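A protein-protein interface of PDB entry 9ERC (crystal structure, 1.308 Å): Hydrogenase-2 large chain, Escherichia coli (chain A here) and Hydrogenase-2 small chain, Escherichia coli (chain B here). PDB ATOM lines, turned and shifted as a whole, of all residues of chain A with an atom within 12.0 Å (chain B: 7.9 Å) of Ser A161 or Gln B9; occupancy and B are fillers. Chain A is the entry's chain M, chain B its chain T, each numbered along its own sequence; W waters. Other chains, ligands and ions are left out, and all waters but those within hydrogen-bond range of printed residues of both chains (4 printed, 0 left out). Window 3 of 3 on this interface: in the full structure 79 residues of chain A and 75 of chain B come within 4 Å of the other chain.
Water W1 lies within hydrogen-bond range of OE1 of Gln A163, NE of Arg B10 and OG of Ser A161. Water W3 lies within hydrogen-bond range of the backbone carbonyl oxygen (O) of Gln A163, the side-chain hydroxyl (OG) of Ser B45, the guanidinium group (NH1) of Arg B10 and the backbone NH (N) of Gly A165. Water W2 lies within hydrogen-bond range of the backbone carbonyl oxygen of Glu B47 (2.8 Å) and the backbone carbonyl oxygen of Gly A165 (3.2 Å). Water W4 lies within hydrogen-bond range of the backbone carbonyl oxygen (O) of Glu B47 (3.4 Å) and the backbone NH (N) of Ile A166 (3.4 Å).
The backbone carbonyl oxygen (O) of Pro B11 sits at hydrogen-bond distance from the backbone NH (N) of Ser B45 (2.8 Å). The side-chain hydroxyl of Ser B45 lies within hydrogen-bond range of the side-chain carboxylate of Glu B47, 2.6 Å away. The side-chain hydroxyl (OH) of Tyr B71 sits at hydrogen-bond distance from the side-chain carboxylate (OE2) of Glu B47 (3.4 Å). The side-chain hydroxyl of Tyr B71 is in hydrogen-bond range of the side-chain amino group of Lys B70 (3.2 Å). The backbone carbonyl oxygen (O) of Leu A158 sits at hydrogen-bond distance from the side-chain hydroxyl (OG) of Ser A161, at 2.7 Å. The side-chain hydroxyl (OG) of Ser A161 is in hydrogen-bond range of the backbone NH (N) of Gln A163.
The backbone carbonyl oxygen (O) of Ser A161 sits at hydrogen-bond distance from the side-chain amide nitrogen (NE2) of Gln B9, 2.8 Å away. The guanidinium group of Arg B10 sits at hydrogen-bond distance from the side-chain hydroxyl of Ser A161 (3.1 Å). The backbone NH (N) of Arg B10 lies within hydrogen-bond range of the side-chain amide oxygen (OE1) of Gln A163 (2.7 Å). The side-chain hydroxyl (OH) of Tyr B71 lies within hydrogen-bond range of the side-chain amide nitrogen (NE2) of Gln A163.
Hydrophobic or aromatic side chains of chain B that line the printed part of chain A: Tyr B71. Of the 19 printed residues of chain A, 4 touch a printed residue of chain B. Hydrophobic or aromatic side chains of chain A within 4 Å of the printed part of chain B: Leu A158.
Ala A160 touches none of the printed residues of chain B. Of the printed residues of chain B, Ser A161 touches Gln B9 (2.8 Å) and Arg B10 (3.1 Å). Of the printed residues of chain B, Gly A162 touches Lys B70. Leu A164 touches none of the printed residues of chain B. Gln B9 touches just these residues of chain A: Ser A161 (2.8 Å) and Gln A163 (3.3 Å). Arg B10 touches just these residues of chain A: Leu A158, Ser A161 and Gln A163. No residue of chain A comes within 4 Å of Pro B11. Of the printed residues of chain A, Lys B70 touches Gly A162. The nearest residue of chain B that does not touch Ser A161 is Lys B70 (6.0 Å). The nearest printed residue of chain A that does not touch Lys B70 is Gln A163 (4.7 Å).
Among the printed residues, merely in contact across the chains: Leu A158 with Arg B10 (3.6 Å), Gly A162 with Lys B70 (3.996 Å), Gln A163 with Gln B9 (3.3 Å) and Gln A163 with Ser B45 (3.6 Å).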
ATOM      1  N   ILE A 119      30.671  -7.565 -23.625  1.00  0.00           N
ATOM      2  CA  ILE A 119      29.781  -8.726 -23.646  1.00  0.00           C
ATOM      3  C   ILE A 119      29.528  -9.220 -25.075  1.00  0.00           C
ATOM      4  O   ILE A 119      29.248 -10.403 -25.249  1.00  0.00           O
ATOM      5  CB  ILE A 119      28.444  -8.472 -22.931  1.00  0.00           C
ATOM      6  CG1 ILE A 119      27.583  -7.460 -23.686  1.00  0.00           C
ATOM      7  CG2 ILE A 119      28.658  -8.084 -21.491  1.00  0.00           C
ATOM      8  CD1 ILE A 119      26.172  -7.358 -23.160  1.00  0.00           C
ATOM      9  N   LEU A 123      30.266 -13.270 -27.105  1.00  0.00           N
ATOM     10  CA  LEU A 123      29.449 -14.101 -27.992  1.00  0.00           C
ATOM     11  C   LEU A 123      30.288 -14.847 -29.027  1.00  0.00           C
ATOM     12  O   LEU A 123      29.865 -15.877 -29.541  1.00  0.00           O
ATOM     13  CB  LEU A 123      28.415 -13.220 -28.680  1.00  0.00           C
ATOM     14  CG  LEU A 123      27.333 -12.674 -27.756  1.00  0.00           C
ATOM     15  CD1 LEU A 123      26.405 -11.756 -28.503  1.00  0.00           C
ATOM     16  CD2 LEU A 123      26.552 -13.824 -27.115  1.00  0.00           C
ATOM     17  N   GLN A 152      27.193 -18.080 -22.062  1.00  0.00           N
ATOM     18  CA  GLN A 152      27.163 -17.530 -23.402  1.00  0.00           C
ATOM     19  C   GLN A 152      25.744 -17.539 -23.954  1.00  0.00           C
ATOM     20  O   GLN A 152      25.317 -16.581 -24.599  1.00  0.00           O
ATOM     21  CB  GLN A 152      28.165 -18.268 -24.287  1.00  0.00           C
ATOM     22  CG  GLN A 152      28.346 -17.617 -25.652  1.00  0.00           C
ATOM     23  CD  GLN A 152      29.353 -18.380 -26.480  1.00  0.00           C
ATOM     24  OE1 GLN A 152      29.198 -19.572 -26.762  1.00  0.00           O
ATOM     25  NE2 GLN A 152      30.443 -17.709 -26.828  1.00  0.00           N
ATOM     26  N   ASN A 153      24.996 -18.625 -23.711  1.00  0.00           N
ATOM     27  CA  ASN A 153      23.628 -18.739 -24.204  1.00  0.00           C
ATOM     28  C   ASN A 153      22.696 -17.722 -23.559  1.00  0.00           C
ATOM     29  O   ASN A 153      21.799 -17.201 -24.204  1.00  0.00           O
ATOM     30  CB  ASN A 153      23.102 -20.168 -24.057  1.00  0.00           C
ATOM     31  CG  ASN A 153      23.775 -21.116 -25.026  1.00  0.00           C
ATOM     32  OD1 ASN A 153      24.315 -20.699 -26.049  1.00  0.00           O
ATOM     33  ND2 ASN A 153      23.715 -22.397 -24.731  1.00  0.00           N
ATOM     34  N   LYS A 154      22.895 -17.400 -22.285  1.00  0.00           N
ATOM     35  CA  LYS A 154      22.100 -16.354 -21.668  1.00  0.00           C
ATOM     36  C   LYS A 154      22.370 -15.003 -22.325  1.00  0.00           C
ATOM     37  O   LYS A 154      21.443 -14.223 -22.506  1.00  0.00           O
ATOM     38  CB  LYS A 154      22.421 -16.214 -20.178  1.00  0.00           C
ATOM     39  CG  LYS A 154      22.003 -17.382 -19.303  1.00  0.00           C
ATOM     40  CD  LYS A 154      22.559 -17.191 -17.906  1.00  0.00           C
ATOM     41  CE  LYS A 154      22.353 -18.372 -16.994  1.00  0.00           C
ATOM     42  NZ  LYS A 154      20.977 -18.380 -16.462  1.00  0.00           N
ATOM     43  N   ILE A 155      23.639 -14.694 -22.629  1.00  0.00           N
ATOM     44  CA  ILE A 155      23.964 -13.434 -23.292  1.00  0.00           C
ATOM     45  C   ILE A 155      23.309 -13.416 -24.679  1.00  0.00           C
ATOM     46  O   ILE A 155      22.717 -12.423 -25.083  1.00  0.00           O
ATOM     47  CB  ILE A 155      25.484 -13.236 -23.457  1.00  0.00           C
ATOM     48  CG1 ILE A 155      26.251 -13.255 -22.134  1.00  0.00           C
ATOM     49  CG2 ILE A 155      25.779 -11.950 -24.239  1.00  0.00           C
ATOM     50  CD1 ILE A 155      27.744 -13.449 -22.331  1.00  0.00           C
ATOM     51  N   LYS A 156      23.502 -14.510 -25.421  1.00  0.00           N
ATOM     52  CA  LYS A 156      22.917 -14.675 -26.743  1.00  0.00           C
ATOM     53  C   LYS A 156      21.415 -14.399 -26.704  1.00  0.00           C
ATOM     54  O   LYS A 156      20.902 -13.663 -27.543  1.00  0.00           O
ATOM     55  CB  LYS A 156      23.266 -16.077 -27.256  1.00  0.00           C
ATOM     56  CG  LYS A 156      22.743 -16.398 -28.643  1.00  0.00           C
ATOM     57  CD  LYS A 156      22.846 -17.865 -29.028  1.00  0.00           C
ATOM     58  CE  LYS A 156      24.182 -18.239 -29.628  1.00  0.00           C
ATOM     59  NZ  LYS A 156      25.277 -18.099 -28.638  1.00  0.00           N
ATOM     60  N   ASP A 157      20.702 -14.991 -25.739  1.00  0.00           N
ATOM     61  CA  ASP A 157      19.261 -14.823 -25.624  1.00  0.00           C
ATOM     62  C   ASP A 157      18.886 -13.381 -25.301  1.00  0.00           C
ATOM     63  O   ASP A 157      17.899 -12.869 -25.829  1.00  0.00           O
ATOM     64  CB  ASP A 157      18.663 -15.726 -24.536  1.00  0.00           C
ATOM     65  CG  ASP A 157      18.694 -17.198 -24.899  1.00  0.00           C
ATOM     66  OD1 ASP A 157      18.914 -17.501 -26.086  1.00  0.00           O
ATOM     67  OD2 ASP A 157      18.520 -18.027 -23.994  1.00  0.00           O
ATOM     68  N   LEU A 158      19.649 -12.750 -24.393  1.00  0.00           N
ATOM     69  CA  LEU A 158      19.393 -11.360 -24.062  1.00  0.00           C
ATOM     70  C   LEU A 158      19.536 -10.499 -25.319  1.00  0.00           C
ATOM     71  O   LEU A 158      18.670  -9.671 -25.603  1.00  0.00           O
ATOM     72  CB  LEU A 158      20.372 -10.938 -22.960  1.00  0.00           C
ATOM     73  CG  LEU A 158      20.310  -9.469 -22.529  1.00  0.00           C
ATOM     74  CD1 LEU A 158      19.132  -9.213 -21.623  1.00  0.00           C
ATOM     75  CD2 LEU A 158      21.602  -9.062 -21.831  1.00  0.00           C
ATOM     76  N   VAL A 159      20.652 -10.668 -26.029  1.00  0.00           N
ATOM     77  CA  VAL A 159      20.916  -9.858 -27.208  1.00  0.00           C
ATOM     78  C   VAL A 159      19.841 -10.121 -28.264  1.00  0.00           C
ATOM     79  O   VAL A 159      19.272  -9.180 -28.808  1.00  0.00           O
ATOM     80  CB  VAL A 159      22.342 -10.111 -27.734  1.00  0.00           C
ATOM     81  CG1 VAL A 159      22.590  -9.431 -29.067  1.00  0.00           C
ATOM     82  CG2 VAL A 159      23.371  -9.652 -26.716  1.00  0.00           C
ATOM     83  N   ALA A 160      19.502 -11.396 -28.475  1.00  0.00           N
ATOM     84  CA  ALA A 160      18.464 -11.784 -29.416  1.00  0.00           C
ATOM     85  C   ALA A 160      17.127 -11.118 -29.115  1.00  0.00           C
ATOM     86  O   ALA A 160      16.391 -10.805 -30.041  1.00  0.00           O
ATOM     87  CB  ALA A 160      18.313 -13.285 -29.446  1.00  0.00           C
ATOM     88  N   SER A 161      16.793 -10.906 -27.846  1.00  0.00           N
ATOM     89  CA  SER A 161      15.500 -10.368 -27.464  1.00  0.00           C
ATOM     90  C   SER A 161      15.350  -8.918 -27.906  1.00  0.00           C
ATOM     91  O   SER A 161      14.247  -8.387 -27.874  1.00  0.00           O
ATOM     92  CB  SER A 161      15.310 -10.446 -25.965  1.00  0.00           C
ATOM     93  OG  SER A 161      16.022  -9.393 -25.312  1.00  0.00           O
ATOM     94  N   GLY A 162      16.474  -8.268 -28.222  1.00  0.00           N
ATOM     95  CA  GLY A 162      16.476  -6.853 -28.544  1.00  0.00           C
ATOM     96  C   GLY A 162      16.257  -5.960 -27.323  1.00  0.00           C
ATOM     97  O   GLY A 162      16.093  -4.757 -27.481  1.00  0.00           O
ATOM     98  N   GLN A 163      16.218  -6.536 -26.110  1.00  0.00           N
ATOM     99  CA  GLN A 163      16.045  -5.754 -24.902  1.00  0.00           C
ATOM    100  C   GLN A 163      17.294  -5.939 -24.041  1.00  0.00           C
ATOM    101  O   GLN A 163      17.335  -6.841 -23.209  1.00  0.00           O
ATOM    102  CB  GLN A 163      14.834  -6.229 -24.102  1.00  0.00           C
ATOM    103  CG  GLN A 163      13.500  -6.087 -24.805  1.00  0.00           C
ATOM    104  CD  GLN A 163      12.395  -6.523 -23.877  1.00  0.00           C
ATOM    105  OE1 GLN A 163      12.216  -7.717 -23.618  1.00  0.00           O
ATOM    106  NE2 GLN A 163      11.675  -5.555 -23.335  1.00  0.00           N
ATOM    107  N   LEU A 164      18.315  -5.101 -24.273  1.00  0.00           N
ATOM    108  CA  LEU A 164      19.608  -5.253 -23.622  1.00  0.00           C
ATOM    109  C   LEU A 164      19.577  -4.723 -22.190  1.00  0.00           C
ATOM    110  O   LEU A 164      20.416  -5.136 -21.386  1.00  0.00           O
ATOM    111  CB  LEU A 164      20.706  -4.540 -24.421  1.00  0.00           C
ATOM    112  CG  LEU A 164      21.330  -5.317 -25.577  1.00  0.00           C
ATOM    113  CD1 LEU A 164      22.032  -6.545 -25.064  1.00  0.00           C
ATOM    114  CD2 LEU A 164      20.274  -5.691 -26.607  1.00  0.00           C
ATOM    115  N   GLY A 165      18.615  -3.868 -21.869  1.00  0.00           N
ATOM    116  CA  GLY A 165      18.427  -3.360 -20.518  1.00  0.00           C
ATOM    117  C   GLY A 165      19.688  -2.669 -19.993  1.00  0.00           C
ATOM    118  O   GLY A 165      20.204  -1.761 -20.634  1.00  0.00           O
ATOM    119  N   ILE A 166      20.229  -3.195 -18.895  1.00  0.00           N
ATOM    120  CA  ILE A 166      21.389  -2.603 -18.247  1.00  0.00           C
ATOM    121  C   ILE A 166      22.625  -2.725 -19.143  1.00  0.00           C
ATOM    122  O   ILE A 166      23.614  -2.032 -18.909  1.00  0.00           O
ATOM    123  CB  ILE A 166      21.626  -3.224 -16.845  1.00  0.00           C
ATOM    124  CG1 ILE A 166      21.910  -4.723 -16.897  1.00  0.00           C
ATOM    125  CG2 ILE A 166      20.495  -2.930 -15.890  1.00  0.00           C
ATOM    126  CD1 ILE A 166      22.672  -5.220 -15.684  1.00  0.00           C
ATOM    127  N   PHE A 167      22.584  -3.598 -20.161  1.00  0.00           N
ATOM    128  CA  PHE A 167      23.702  -3.766 -21.063  1.00  0.00           C
ATOM    129  C   PHE A 167      23.578  -2.894 -22.320  1.00  0.00           C
ATOM    130  O   PHE A 167      24.482  -2.882 -23.159  1.00  0.00           O
ATOM    131  CB  PHE A 167      23.819  -5.241 -21.443  1.00  0.00           C
ATOM    132  CG  PHE A 167      24.052  -6.118 -20.246  1.00  0.00           C
ATOM    133  CD1 PHE A 167      25.311  -6.188 -19.667  1.00  0.00           C
ATOM    134  CD2 PHE A 167      22.997  -6.777 -19.632  1.00  0.00           C
ATOM    135  CE1 PHE A 167      25.526  -6.974 -18.546  1.00  0.00           C
ATOM    136  CE2 PHE A 167      23.212  -7.545 -18.495  1.00  0.00           C
ATOM    137  CZ  PHE A 167      24.476  -7.640 -17.953  1.00  0.00           C
ATOM    138  N   ALA A 168      22.490  -2.154 -22.470  1.00  0.00           N
ATOM    139  CA  ALA A 168      22.270  -1.402 -23.706  1.00  0.00           C
ATOM    140  C   ALA A 168      23.255  -0.242 -23.802  1.00  0.00           C
ATOM    141  O   ALA A 168      23.494   0.445 -22.818  1.00  0.00           O
ATOM    142  CB  ALA A 168      20.860  -0.879 -23.738  1.00  0.00           C
ATOM    143  N   GLN B   9       9.495 -11.039 -25.013  1.00  0.00           N
ATOM    144  CA  GLN B   9       9.728  -9.653 -24.517  1.00  0.00           C
ATOM    145  C   GLN B   9       9.385  -9.575 -23.035  1.00  0.00           C
ATOM    146  O   GLN B   9       8.415 -10.178 -22.592  1.00  0.00           O
ATOM    147  CB  GLN B   9       8.896  -8.652 -25.313  1.00  0.00           C
ATOM    148  CG  GLN B   9       9.282  -8.656 -26.785  1.00  0.00           C
ATOM    149  CD  GLN B   9      10.697  -8.186 -27.018  1.00  0.00           C
ATOM    150  OE1 GLN B   9      11.012  -7.006 -26.899  1.00  0.00           O
ATOM    151  NE2 GLN B   9      11.572  -9.108 -27.384  1.00  0.00           N
ATOM    152  N   ARG B  10      10.187  -8.833 -22.268  1.00  0.00           N
ATOM    153  CA  ARG B  10       9.975  -8.735 -20.832  1.00  0.00           C
ATOM    154  C   ARG B  10       9.442  -7.353 -20.496  1.00  0.00           C
ATOM    155  O   ARG B  10       9.738  -6.360 -21.171  1.00  0.00           O
ATOM    156  CB  ARG B  10      11.288  -9.020 -20.123  1.00  0.00           C
ATOM    157  CG  ARG B  10      11.709 -10.479 -20.141  1.00  0.00           C
ATOM    158  CD  ARG B  10      13.180 -10.651 -19.845  1.00  0.00           C
ATOM    159  NE  ARG B  10      13.984 -10.302 -21.006  1.00  0.00           N
ATOM    160  CZ  ARG B  10      14.956  -9.406 -21.055  1.00  0.00           C
ATOM    161  NH1 ARG B  10      15.354  -8.770 -19.967  1.00  0.00           N
ATOM    162  NH2 ARG B  10      15.560  -9.182 -22.207  1.00  0.00           N
ATOM    163  N   PRO B  11       8.613  -7.230 -19.452  1.00  0.00           N
ATOM    164  CA  PRO B  11       8.040  -5.952 -19.069  1.00  0.00           C
ATOM    165  C   PRO B  11       9.114  -4.949 -18.650  1.00  0.00           C
ATOM    166  O   PRO B  11      10.023  -5.251 -17.873  1.00  0.00           O
ATOM    167  CB  PRO B  11       7.080  -6.218 -17.910  1.00  0.00           C
ATOM    168  CG  PRO B  11       7.205  -7.694 -17.608  1.00  0.00           C
ATOM    169  CD  PRO B  11       8.122  -8.335 -18.621  1.00  0.00           C
ATOM    170  N   PRO B  12       9.055  -3.726 -19.214  1.00  0.00           N
ATOM    171  CA  PRO B  12      10.094  -2.730 -18.976  1.00  0.00           C
ATOM    172  C   PRO B  12       9.916  -2.010 -17.642  1.00  0.00           C
ATOM    173  O   PRO B  12       8.797  -1.739 -17.176  1.00  0.00           O
ATOM    174  CB  PRO B  12       9.916  -1.816 -20.202  1.00  0.00           C
ATOM    175  CG  PRO B  12       8.433  -1.846 -20.456  1.00  0.00           C
ATOM    176  CD  PRO B  12       8.040  -3.285 -20.195  1.00  0.00           C
ATOM    177  N   LEU B  41      17.383 -10.686 -16.140  1.00  0.00           N
ATOM    178  CA  LEU B  41      17.529 -11.500 -17.342  1.00  0.00           C
ATOM    179  C   LEU B  41      16.201 -12.153 -17.741  1.00  0.00           C
ATOM    180  O   LEU B  41      16.014 -12.423 -18.923  1.00  0.00           O
ATOM    181  CB  LEU B  41      18.608 -12.568 -17.157  1.00  0.00           C
ATOM    182  CG  LEU B  41      20.052 -12.079 -16.985  1.00  0.00           C
ATOM    183  CD1 LEU B  41      21.000 -13.248 -16.922  1.00  0.00           C
ATOM    184  CD2 LEU B  41      20.478 -11.136 -18.115  1.00  0.00           C
ATOM    185  N   GLU B  42      15.317 -12.457 -16.776  1.00  0.00           N
ATOM    186  CA  GLU B  42      14.122 -13.254 -17.042  1.00  0.00           C
ATOM    187  C   GLU B  42      12.828 -12.520 -16.727  1.00  0.00           C
ATOM    188  O   GLU B  42      11.879 -12.614 -17.495  1.00  0.00           O
ATOM    189  CB  GLU B  42      14.052 -14.548 -16.226  1.00  0.00           C
ATOM    190  CG  GLU B  42      15.318 -15.362 -16.183  1.00  0.00           C
ATOM    191  CD  GLU B  42      15.771 -15.956 -17.495  1.00  0.00           C
ATOM    192  OE1 GLU B  42      14.910 -16.229 -18.363  1.00  0.00           O
ATOM    193  OE2 GLU B  42      16.993 -16.122 -17.653  1.00  0.00           O
ATOM    194  N   THR B  43      12.731 -11.826 -15.597  1.00  0.00           N
ATOM    195  CA  THR B  43      11.456 -11.308 -15.132  1.00  0.00           C
ATOM    196  C   THR B  43      11.079  -9.978 -15.785  1.00  0.00           C
ATOM    197  O   THR B  43       9.931  -9.792 -16.175  1.00  0.00           O
ATOM    198  CB  THR B  43      11.457 -11.122 -13.615  1.00  0.00           C
ATOM    199  OG1 THR B  43      11.926 -12.339 -13.054  1.00  0.00           O
ATOM    200  CG2 THR B  43      10.096 -10.777 -13.064  1.00  0.00           C
ATOM    201  N   ILE B  44      12.040  -9.037 -15.853  1.00  0.00           N
ATOM    202  CA  ILE B  44      11.781  -7.694 -16.369  1.00  0.00           C
ATOM    203  C   ILE B  44      12.881  -7.377 -17.374  1.00  0.00           C
ATOM    204  O   ILE B  44      13.876  -8.090 -17.496  1.00  0.00           O
ATOM    205  CB  ILE B  44      11.714  -6.617 -15.251  1.00  0.00           C
ATOM    206  CG1 ILE B  44      13.070  -6.483 -14.550  1.00  0.00           C
ATOM    207  CG2 ILE B  44      10.574  -6.913 -14.304  1.00  0.00           C
ATOM    208  CD1 ILE B  44      13.216  -5.298 -13.623  1.00  0.00           C
ATOM    209  N   SER B  45      12.670  -6.274 -18.094  1.00  0.00           N
ATOM    210  CA  SER B  45      13.758  -5.587 -18.751  1.00  0.00           C
ATOM    211  C   SER B  45      14.030  -4.302 -17.978  1.00  0.00           C
ATOM    212  O   SER B  45      13.193  -3.406 -17.954  1.00  0.00           O
ATOM    213  CB  SER B  45      13.473  -5.277 -20.207  1.00  0.00           C
ATOM    214  OG  SER B  45      14.644  -4.742 -20.802  1.00  0.00           O
ATOM    215  N   GLU B  47      15.351  -1.216 -18.048  1.00  0.00           N
ATOM    216  CA  GLU B  47      15.704  -0.325 -19.144  1.00  0.00           C
ATOM    217  C   GLU B  47      16.568   0.839 -18.656  1.00  0.00           C
ATOM    218  O   GLU B  47      17.341   1.407 -19.421  1.00  0.00           O
ATOM    219  CB  GLU B  47      14.417   0.229 -19.759  1.00  0.00           C
ATOM    220  CG  GLU B  47      13.611  -0.829 -20.479  1.00  0.00           C
ATOM    221  CD  GLU B  47      14.318  -1.346 -21.713  1.00  0.00           C
ATOM    222  OE1 GLU B  47      14.987  -0.533 -22.350  1.00  0.00           O
ATOM    223  OE2 GLU B  47      14.122  -2.502 -22.080  1.00  0.00           O
ATOM    224  N   LYS B  70       9.941   4.266 -26.592  1.00  0.00           N
ATOM    225  CA  LYS B  70       9.620   2.913 -27.015  1.00  0.00           C
ATOM    226  C   LYS B  70       8.530   2.286 -26.139  1.00  0.00           C
ATOM    227  O   LYS B  70       7.690   1.559 -26.663  1.00  0.00           O
ATOM    228  CB  LYS B  70      10.864   2.024 -27.016  1.00  0.00           C
ATOM    229  CG  LYS B  70      10.629   0.598 -27.499  1.00  0.00           C
ATOM    230  CD  LYS B  70      11.892  -0.224 -27.645  1.00  0.00           C
ATOM    231  CE  LYS B  70      11.599  -1.664 -28.010  1.00  0.00           C
ATOM    232  NZ  LYS B  70      12.775  -2.556 -27.817  1.00  0.00           N
ATOM    233  N   TYR B  71       8.533   2.538 -24.823  1.00  0.00           N
ATOM    234  CA  TYR B  71       7.649   1.829 -23.905  1.00  0.00           C
ATOM    235  C   TYR B  71       6.614   2.746 -23.265  1.00  0.00           C
ATOM    236  O   TYR B  71       6.024   2.403 -22.241  1.00  0.00           O
ATOM    237  CB  TYR B  71       8.466   1.109 -22.836  1.00  0.00           C
ATOM    238  CG  TYR B  71       9.418   0.072 -23.363  1.00  0.00           C
ATOM    239  CD1 TYR B  71       8.951  -1.104 -23.932  1.00  0.00           C
ATOM    240  CD2 TYR B  71      10.782   0.246 -23.284  1.00  0.00           C
ATOM    241  CE1 TYR B  71       9.816  -2.077 -24.408  1.00  0.00           C
ATOM    242  CE2 TYR B  71      11.656  -0.715 -23.747  1.00  0.00           C
ATOM    243  CZ  TYR B  71      11.178  -1.883 -24.316  1.00  0.00           C
ATOM    244  OH  TYR B  71      12.068  -2.837 -24.756  1.00  0.00           O
HETATM  245  O   HOH W   1      13.031 -10.184 -23.791  1.00  0.00           O
HETATM  246  O   HOH W   2      18.278   0.483 -21.837  1.00  0.00           O
HETATM  247  O   HOH W   3      16.903  -6.331 -20.666  1.00  0.00           O
HETATM  248  O   HOH W   4      19.567  -0.168 -17.427  1.00  0.00           O
